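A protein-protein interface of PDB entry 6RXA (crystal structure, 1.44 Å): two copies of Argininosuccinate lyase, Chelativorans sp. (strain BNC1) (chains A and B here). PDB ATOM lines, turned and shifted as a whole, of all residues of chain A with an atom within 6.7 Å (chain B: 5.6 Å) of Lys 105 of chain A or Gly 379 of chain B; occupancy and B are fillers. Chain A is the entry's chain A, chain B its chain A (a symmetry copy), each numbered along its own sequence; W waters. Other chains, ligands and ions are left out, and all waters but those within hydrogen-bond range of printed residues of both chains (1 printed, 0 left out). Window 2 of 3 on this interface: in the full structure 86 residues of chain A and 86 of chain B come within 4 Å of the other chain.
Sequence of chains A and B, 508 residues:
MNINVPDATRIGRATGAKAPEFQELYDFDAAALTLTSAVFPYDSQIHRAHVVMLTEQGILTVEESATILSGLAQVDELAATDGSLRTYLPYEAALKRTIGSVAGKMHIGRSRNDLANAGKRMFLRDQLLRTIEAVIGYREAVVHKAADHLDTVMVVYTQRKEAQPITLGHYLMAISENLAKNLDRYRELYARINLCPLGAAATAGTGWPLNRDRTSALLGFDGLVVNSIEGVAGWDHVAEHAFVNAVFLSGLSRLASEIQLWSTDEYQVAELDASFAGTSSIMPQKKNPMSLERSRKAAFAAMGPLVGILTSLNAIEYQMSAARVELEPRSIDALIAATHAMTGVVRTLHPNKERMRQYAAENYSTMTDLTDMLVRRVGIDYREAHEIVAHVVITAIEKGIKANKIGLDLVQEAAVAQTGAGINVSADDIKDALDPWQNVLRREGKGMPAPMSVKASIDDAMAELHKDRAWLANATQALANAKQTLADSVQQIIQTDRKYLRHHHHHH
Of the 17 printed residues of chain A, 4 touch a printed residue of chain B. Printed residues of chain A that touch a printed residue of chain B: Ser 101, Gly 104, Lys 105 and Ile 108. Among the printed residues, 5 pairs touch across the chains. Among the printed residues, no Asp or Glu carboxylate lies within 4 Å of a Lys or Arg side-chain nitrogen of the other chain.
Of chain A, only Lys 105 comes within 4 Å of Gly 379 of chain B. Of the printed residues of chain A, Asp 381 of chain B touches Ser 101 (3.2 Å) and Gly 104 (3.8 Å). Printed residues of chain B within 4 Å of Gly 104 of chain A: Asp 381 (3.8 Å) and Tyr 382 (3.5 Å). Printed residues of chain B within 4 Å of Ser 101 of chain A: Asp 381 (3.2 Å). Of the printed residues of chain B, Ile 108 of chain A touches Val 375 (3.95 Å). Glu 92 of chain A touches none of the printed residues of chain B. Leu 54 of chain A touches none of the printed residues of chain B. The nearest residue of chain B that does not touch Lys 105 of chain A is Asp 381 of chain B (4.1 Å). The nearest printed residue of chain B that does not touch Gly 104 of chain A is Ile 380 of chain B (7.0 Å).
Water W1 bridges the side-chain carboxylate (OD2) of Asp 381 of chain B (2.9 Å) and the backbone carbonyl oxygen (O) of Ser 101 of chain A (3.2 Å).
No position is printed for both chains. Of the 5 pairs that touch across the chains among the printed residues, none has its exchanged pair printed and touching as well.
The side-chain amino group (NZ) of Lys 105 of chain A is in salt-bridge range of the side-chain carboxylate (OE2) of Glu 64 of chain A (2.7 Å). NE2 of His 50 of chain A is in hydrogen-bond range of O of Ile 108 of chain A (2.8 Å).
Asp 381 of chain B touches Ser 101 of chain A (CB to O, 3.2 Å). CA of Gly 104 of chain A touches OD2 of Asp 381 of chain B, at 3.8 Å. Gly 104 of chain A touches Tyr 382 of chain B (O to CB, 3.5 Å). Gly 379 of chain B touches Lys 105 of chain A. Ile 108 of chain A touches Val 375 of chain B (CD1 to CG1, 3.95 Å).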
ATOM      1  N   HIS A  50      18.232 -22.119   2.821  1.00  0.00           N
ATOM      2  CA  HIS A  50      18.312 -21.023   3.778  1.00  0.00           C
ATOM      3  C   HIS A  50      18.276 -19.684   3.059  1.00  0.00           C
ATOM      4  O   HIS A  50      17.536 -18.772   3.452  1.00  0.00           O
ATOM      5  CB  HIS A  50      19.587 -21.174   4.604  1.00  0.00           C
ATOM      6  CG  HIS A  50      19.731 -20.136   5.664  1.00  0.00           C
ATOM      7  ND1 HIS A  50      18.969 -20.140   6.814  1.00  0.00           N
ATOM      8  CD2 HIS A  50      20.546 -19.061   5.749  1.00  0.00           C
ATOM      9  CE1 HIS A  50      19.313 -19.104   7.560  1.00  0.00           C
ATOM     10  NE2 HIS A  50      20.260 -18.430   6.935  1.00  0.00           N
ATOM     11  N   VAL A  51      19.046 -19.558   1.975  1.00  0.00           N
ATOM     12  CA  VAL A  51      19.100 -18.313   1.210  1.00  0.00           C
ATOM     13  C   VAL A  51      17.752 -17.990   0.573  1.00  0.00           C
ATOM     14  O   VAL A  51      17.312 -16.836   0.589  1.00  0.00           O
ATOM     15  CB  VAL A  51      20.242 -18.389   0.180  1.00  0.00           C
ATOM     16  CG1 VAL A  51      20.097 -17.311  -0.867  1.00  0.00           C
ATOM     17  CG2 VAL A  51      21.591 -18.289   0.882  1.00  0.00           C
ATOM     18  N   LEU A  54      15.584 -16.700   3.308  1.00  0.00           N
ATOM     19  CA  LEU A  54      15.935 -15.335   3.678  1.00  0.00           C
ATOM     20  C   LEU A  54      15.402 -14.348   2.656  1.00  0.00           C
ATOM     21  O   LEU A  54      15.064 -13.209   3.001  1.00  0.00           O
ATOM     22  CB  LEU A  54      17.442 -15.157   3.775  1.00  0.00           C
ATOM     23  CG  LEU A  54      18.201 -15.891   4.865  1.00  0.00           C
ATOM     24  CD1 LEU A  54      19.677 -15.564   4.776  1.00  0.00           C
ATOM     25  CD2 LEU A  54      17.667 -15.513   6.233  1.00  0.00           C
ATOM     26  N   ILE A  59      15.095 -10.547   4.104  1.00  0.00           N
ATOM     27  CA  ILE A  59      16.397 -10.347   4.732  1.00  0.00           C
ATOM     28  C   ILE A  59      17.468 -10.154   3.669  1.00  0.00           C
ATOM     29  O   ILE A  59      18.387  -9.340   3.830  1.00  0.00           O
ATOM     30  CB  ILE A  59      16.698 -11.519   5.683  1.00  0.00           C
ATOM     31  CG1 ILE A  59      15.693 -11.487   6.844  1.00  0.00           C
ATOM     32  CG2 ILE A  59      18.115 -11.452   6.192  1.00  0.00           C
ATOM     33  CD1 ILE A  59      15.706 -12.721   7.713  1.00  0.00           C
ATOM     34  N   LEU A  60      17.362 -10.883   2.563  1.00  0.00           N
ATOM     35  CA  LEU A  60      18.201 -10.673   1.396  1.00  0.00           C
ATOM     36  C   LEU A  60      17.339 -10.129   0.272  1.00  0.00           C
ATOM     37  O   LEU A  60      16.177 -10.524   0.125  1.00  0.00           O
ATOM     38  CB  LEU A  60      18.820 -11.981   0.899  1.00  0.00           C
ATOM     39  CG  LEU A  60      19.727 -12.738   1.861  1.00  0.00           C
ATOM     40  CD1 LEU A  60      20.146 -14.062   1.218  1.00  0.00           C
ATOM     41  CD2 LEU A  60      20.952 -11.927   2.240  1.00  0.00           C
ATOM     42  N   GLU A  64      20.952  -9.842  -4.101  1.00  0.00           N
ATOM     43  CA  GLU A  64      21.921 -10.496  -3.227  1.00  0.00           C
ATOM     44  C   GLU A  64      21.758 -12.005  -3.291  1.00  0.00           C
ATOM     45  O   GLU A  64      22.745 -12.750  -3.379  1.00  0.00           O
ATOM     46  CB  GLU A  64      21.718 -10.030  -1.785  1.00  0.00           C
ATOM     47  CG  GLU A  64      22.133  -8.585  -1.536  1.00  0.00           C
ATOM     48  CD  GLU A  64      21.750  -8.094  -0.151  1.00  0.00           C
ATOM     49  OE1 GLU A  64      20.672  -8.484   0.350  1.00  0.00           O
ATOM     50  OE2 GLU A  64      22.524  -7.306   0.429  1.00  0.00           O
ATOM     51  N   ILE A  68      24.588 -14.826  -4.456  1.00  0.00           N
ATOM     52  CA  ILE A  68      24.974 -15.928  -3.583  1.00  0.00           C
ATOM     53  C   ILE A  68      24.701 -17.271  -4.255  1.00  0.00           C
ATOM     54  O   ILE A  68      25.576 -18.141  -4.314  1.00  0.00           O
ATOM     55  CB  ILE A  68      24.244 -15.810  -2.233  1.00  0.00           C
ATOM     56  CG1 ILE A  68      24.739 -14.577  -1.470  1.00  0.00           C
ATOM     57  CG2 ILE A  68      24.464 -17.068  -1.399  1.00  0.00           C
ATOM     58  CD1 ILE A  68      23.874 -14.178  -0.288  1.00  0.00           C
ATOM     59  N   GLU A  92      32.594 -21.135   2.979  1.00  0.00           N
ATOM     60  CA  GLU A  92      32.155 -19.748   2.975  1.00  0.00           C
ATOM     61  C   GLU A  92      33.269 -18.831   2.494  1.00  0.00           C
ATOM     62  O   GLU A  92      33.015 -17.860   1.775  1.00  0.00           O
ATOM     63  CB  GLU A  92      31.689 -19.343   4.376  1.00  0.00           C
ATOM     64  CG  GLU A  92      30.903 -18.030   4.369  1.00  0.00           C
ATOM     65  CD  GLU A  92      30.792 -17.378   5.739  1.00  0.00           C
ATOM     66  OE1 GLU A  92      31.590 -16.459   6.017  1.00  0.00           O
ATOM     67  OE2 GLU A  92      29.908 -17.769   6.533  1.00  0.00           O
ATOM     68  N   SER A 101      32.061  -9.983  -0.687  1.00  0.00           N
ATOM     69  CA  SER A 101      31.709 -10.013   0.725  1.00  0.00           C
ATOM     70  C   SER A 101      30.255 -10.397   0.986  1.00  0.00           C
ATOM     71  O   SER A 101      29.948 -10.848   2.094  1.00  0.00           O
ATOM     72  CB  SER A 101      32.020  -8.657   1.354  1.00  0.00           C
ATOM     73  OG  SER A 101      31.260  -7.639   0.724  1.00  0.00           O
ATOM     74  N   VAL A 102      29.357 -10.228   0.011  1.00  0.00           N
ATOM     75  CA  VAL A 102      27.966 -10.646   0.182  1.00  0.00           C
ATOM     76  C   VAL A 102      27.850 -12.124   0.536  1.00  0.00           C
ATOM     77  O   VAL A 102      26.819 -12.557   1.067  1.00  0.00           O
ATOM     78  CB  VAL A 102      27.146 -10.294  -1.081  1.00  0.00           C
ATOM     79  CG1 VAL A 102      27.493 -11.223  -2.238  1.00  0.00           C
ATOM     80  CG2 VAL A 102      25.648 -10.337  -0.770  1.00  0.00           C
ATOM     81  N   ALA A 103      28.887 -12.914   0.247  1.00  0.00           N
ATOM     82  CA  ALA A 103      28.895 -14.320   0.639  1.00  0.00           C
ATOM     83  C   ALA A 103      28.587 -14.482   2.117  1.00  0.00           C
ATOM     84  O   ALA A 103      27.920 -15.439   2.521  1.00  0.00           O
ATOM     85  CB  ALA A 103      30.264 -14.934   0.342  1.00  0.00           C
ATOM     86  N   GLY A 104      29.095 -13.567   2.945  1.00  0.00           N
ATOM     87  CA  GLY A 104      28.901 -13.665   4.381  1.00  0.00           C
ATOM     88  C   GLY A 104      27.455 -13.571   4.810  1.00  0.00           C
ATOM     89  O   GLY A 104      27.095 -14.049   5.896  1.00  0.00           O
ATOM     90  N   LYS A 105      26.606 -12.979   3.979  1.00  0.00           N
ATOM     91  CA  LYS A 105      25.208 -12.832   4.345  1.00  0.00           C
ATOM     92  C   LYS A 105      24.456 -14.147   4.319  1.00  0.00           C
ATOM     93  O   LYS A 105      23.351 -14.214   4.865  1.00  0.00           O
ATOM     94  CB  LYS A 105      24.522 -11.817   3.425  1.00  0.00           C
ATOM     95  CG  LYS A 105      24.998 -10.395   3.653  1.00  0.00           C
ATOM     96  CD  LYS A 105      24.021  -9.378   3.070  1.00  0.00           C
ATOM     97  CE  LYS A 105      24.440  -7.958   3.402  1.00  0.00           C
ATOM     98  NZ  LYS A 105      23.396  -6.981   2.990  1.00  0.00           N
ATOM     99  N   MET A 106      25.001 -15.190   3.683  1.00  0.00           N
ATOM    100  CA  MET A 106      24.285 -16.458   3.709  1.00  0.00           C
ATOM    101  C   MET A 106      24.255 -17.068   5.108  1.00  0.00           C
ATOM    102  O   MET A 106      23.493 -18.008   5.339  1.00  0.00           O
ATOM    103  CB  MET A 106      24.847 -17.467   2.696  1.00  0.00           C
ATOM    104  CG  MET A 106      26.154 -18.165   3.076  1.00  0.00           C
ATOM    105  SD  MET A 106      26.277 -19.774   2.234  1.00  0.00           S
ATOM    106  CE  MET A 106      28.011 -20.132   2.487  1.00  0.00           C
ATOM    107  N   HIS A 107      25.059 -16.562   6.037  1.00  0.00           N
ATOM    108  CA  HIS A 107      25.078 -17.095   7.394  1.00  0.00           C
ATOM    109  C   HIS A 107      24.166 -16.327   8.339  1.00  0.00           C
ATOM    110  O   HIS A 107      24.098 -16.665   9.522  1.00  0.00           O
ATOM    111  CB  HIS A 107      26.502 -17.101   7.945  1.00  0.00           C
ATOM    112  CG  HIS A 107      26.788 -18.240   8.881  1.00  0.00           C
ATOM    113  ND1 HIS A 107      26.484 -19.548   8.575  1.00  0.00           N
ATOM    114  CD2 HIS A 107      27.355 -18.265  10.110  1.00  0.00           C
ATOM    115  CE1 HIS A 107      26.852 -20.331   9.575  1.00  0.00           C
ATOM    116  NE2 HIS A 107      27.392 -19.579  10.513  1.00  0.00           N
ATOM    117  N   ILE A 108      23.458 -15.304   7.851  1.00  0.00           N
ATOM    118  CA  ILE A 108      22.550 -14.560   8.716  1.00  0.00           C
ATOM    119  C   ILE A 108      21.529 -15.503   9.337  1.00  0.00           C
ATOM    120  O   ILE A 108      20.861 -16.281   8.640  1.00  0.00           O
ATOM    121  CB  ILE A 108      21.880 -13.423   7.928  1.00  0.00           C
ATOM    122  CG1 ILE A 108      22.892 -12.310   7.645  1.00  0.00           C
ATOM    123  CG2 ILE A 108      20.683 -12.893   8.706  1.00  0.00           C
ATOM    124  CD1 ILE A 108      22.394 -11.265   6.635  1.00  0.00           C
ATOM    125  N   GLY A 109      21.392 -15.432  10.657  1.00  0.00           N
ATOM    126  CA  GLY A 109      20.405 -16.228  11.361  1.00  0.00           C
ATOM    127  C   GLY A 109      20.718 -17.703  11.495  1.00  0.00           C
ATOM    128  O   GLY A 109      19.831 -18.478  11.846  1.00  0.00           O
ATOM    129  N   LEU B 374      24.981  -4.793  14.008  1.00  0.00           N
ATOM    130  CA  LEU B 374      25.807  -4.140  13.001  1.00  0.00           C
ATOM    131  C   LEU B 374      25.335  -4.501  11.595  1.00  0.00           C
ATOM    132  O   LEU B 374      25.170  -3.628  10.741  1.00  0.00           O
ATOM    133  CB  LEU B 374      27.274  -4.515  13.173  1.00  0.00           C
ATOM    134  CG  LEU B 374      27.925  -4.196  14.517  1.00  0.00           C
ATOM    135  CD1 LEU B 374      29.413  -4.553  14.471  1.00  0.00           C
ATOM    136  CD2 LEU B 374      27.717  -2.761  14.911  1.00  0.00           C
ATOM    137  N   VAL B 375      25.101  -5.794  11.349  1.00  0.00           N
ATOM    138  CA  VAL B 375      24.596  -6.227  10.046  1.00  0.00           C
ATOM    139  C   VAL B 375      23.284  -5.524   9.724  1.00  0.00           C
ATOM    140  O   VAL B 375      23.094  -4.993   8.625  1.00  0.00           O
ATOM    141  CB  VAL B 375      24.424  -7.757  10.034  1.00  0.00           C
ATOM    142  CG1 VAL B 375      23.714  -8.211   8.768  1.00  0.00           C
ATOM    143  CG2 VAL B 375      25.773  -8.439  10.180  1.00  0.00           C
ATOM    144  N   ARG B 376      22.357  -5.519  10.682  1.00  0.00           N
ATOM    145  CA  ARG B 376      21.025  -4.977  10.441  1.00  0.00           C
ATOM    146  C   ARG B 376      21.059  -3.465  10.268  1.00  0.00           C
ATOM    147  O   ARG B 376      20.340  -2.919   9.422  1.00  0.00           O
ATOM    148  CB  ARG B 376      20.120  -5.362  11.612  1.00  0.00           C
ATOM    149  CG  ARG B 376      18.641  -5.124  11.393  1.00  0.00           C
ATOM    150  CD  ARG B 376      17.835  -5.514  12.640  1.00  0.00           C
ATOM    151  NE  ARG B 376      17.867  -6.953  12.910  1.00  0.00           N
ATOM    152  CZ  ARG B 376      18.502  -7.532  13.933  1.00  0.00           C
ATOM    153  NH1 ARG B 376      19.179  -6.809  14.820  1.00  0.00           N
ATOM    154  NH2 ARG B 376      18.455  -8.852  14.067  1.00  0.00           N
ATOM    155  N   ARG B 377      21.899  -2.771  11.043  1.00  0.00           N
ATOM    156  CA  ARG B 377      21.888  -1.310  11.039  1.00  0.00           C
ATOM    157  C   ARG B 377      22.723  -0.718   9.908  1.00  0.00           C
ATOM    158  O   ARG B 377      22.298   0.257   9.276  1.00  0.00           O
ATOM    159  CB  ARG B 377      22.387  -0.776  12.383  1.00  0.00           C
ATOM    160  CG  ARG B 377      21.437  -1.035  13.549  1.00  0.00           C
ATOM    161  CD  ARG B 377      20.274  -0.046  13.577  1.00  0.00           C
ATOM    162  NE  ARG B 377      20.714   1.308  13.904  1.00  0.00           N
ATOM    163  CZ  ARG B 377      19.915   2.370  13.946  1.00  0.00           C
ATOM    164  NH1 ARG B 377      18.621   2.246  13.680  1.00  0.00           N
ATOM    165  NH2 ARG B 377      20.412   3.562  14.253  1.00  0.00           N
ATOM    166  N   VAL B 378      23.915  -1.259   9.649  1.00  0.00           N
ATOM    167  CA  VAL B 378      24.809  -0.698   8.637  1.00  0.00           C
ATOM    168  C   VAL B 378      24.965  -1.593   7.416  1.00  0.00           C
ATOM    169  O   VAL B 378      25.648  -1.200   6.457  1.00  0.00           O
ATOM    170  CB  VAL B 378      26.181  -0.297   9.217  1.00  0.00           C
ATOM    171  CG1 VAL B 378      25.996   0.567  10.465  1.00  0.00           C
ATOM    172  CG2 VAL B 378      27.023  -1.517   9.533  1.00  0.00           C
ATOM    173  N   GLY B 379      24.370  -2.783   7.420  1.00  0.00           N
ATOM    174  CA  GLY B 379      24.308  -3.604   6.230  1.00  0.00           C
ATOM    175  C   GLY B 379      25.575  -4.336   5.858  1.00  0.00           C
ATOM    176  O   GLY B 379      25.624  -4.930   4.774  1.00  0.00           O
ATOM    177  N   ILE B 380      26.610  -4.308   6.708  1.00  0.00           N
ATOM    178  CA  ILE B 380      27.794  -5.123   6.450  1.00  0.00           C
ATOM    179  C   ILE B 380      27.409  -6.605   6.492  1.00  0.00           C
ATOM    180  O   ILE B 380      26.357  -6.986   7.015  1.00  0.00           O
ATOM    181  CB  ILE B 380      28.923  -4.821   7.446  1.00  0.00           C
ATOM    182  CG1 ILE B 380      28.479  -5.080   8.883  1.00  0.00           C
ATOM    183  CG2 ILE B 380      29.367  -3.366   7.331  1.00  0.00           C
ATOM    184  CD1 ILE B 380      29.523  -4.656   9.917  1.00  0.00           C
ATOM    185  N   ASP B 381      28.273  -7.448   5.921  1.00  0.00           N
ATOM    186  CA  ASP B 381      28.017  -8.886   5.924  1.00  0.00           C
ATOM    187  C   ASP B 381      28.354  -9.472   7.291  1.00  0.00           C
ATOM    188  O   ASP B 381      29.067  -8.862   8.091  1.00  0.00           O
ATOM    189  CB  ASP B 381      28.835  -9.598   4.840  1.00  0.00           C
ATOM    190  CG  ASP B 381      30.321  -9.609   5.140  1.00  0.00           C
ATOM    191  OD1 ASP B 381      30.987  -8.570   4.925  1.00  0.00           O
ATOM    192  OD2 ASP B 381      30.817 -10.658   5.606  1.00  0.00           O
ATOM    193  N   TYR B 382      27.839 -10.682   7.553  1.00  0.00           N
ATOM    194  CA  TYR B 382      27.954 -11.241   8.894  1.00  0.00           C
ATOM    195  C   TYR B 382      29.410 -11.528   9.259  1.00  0.00           C
ATOM    196  O   TYR B 382      29.806 -11.380  10.422  1.00  0.00           O
ATOM    197  CB  TYR B 382      27.109 -12.507   9.057  1.00  0.00           C
ATOM    198  CG  TYR B 382      26.968 -12.800  10.536  1.00  0.00           C
ATOM    199  CD1 TYR B 382      25.987 -12.168  11.281  1.00  0.00           C
ATOM    200  CD2 TYR B 382      27.875 -13.612  11.200  1.00  0.00           C
ATOM    201  CE1 TYR B 382      25.879 -12.369  12.642  1.00  0.00           C
ATOM    202  CE2 TYR B 382      27.779 -13.819  12.568  1.00  0.00           C
ATOM    203  CZ  TYR B 382      26.771 -13.193  13.280  1.00  0.00           C
ATOM    204  OH  TYR B 382      26.647 -13.362  14.638  1.00  0.00           O
HETATM  205  O   HOH W   1      32.405 -12.175   3.637  1.00  0.00           O
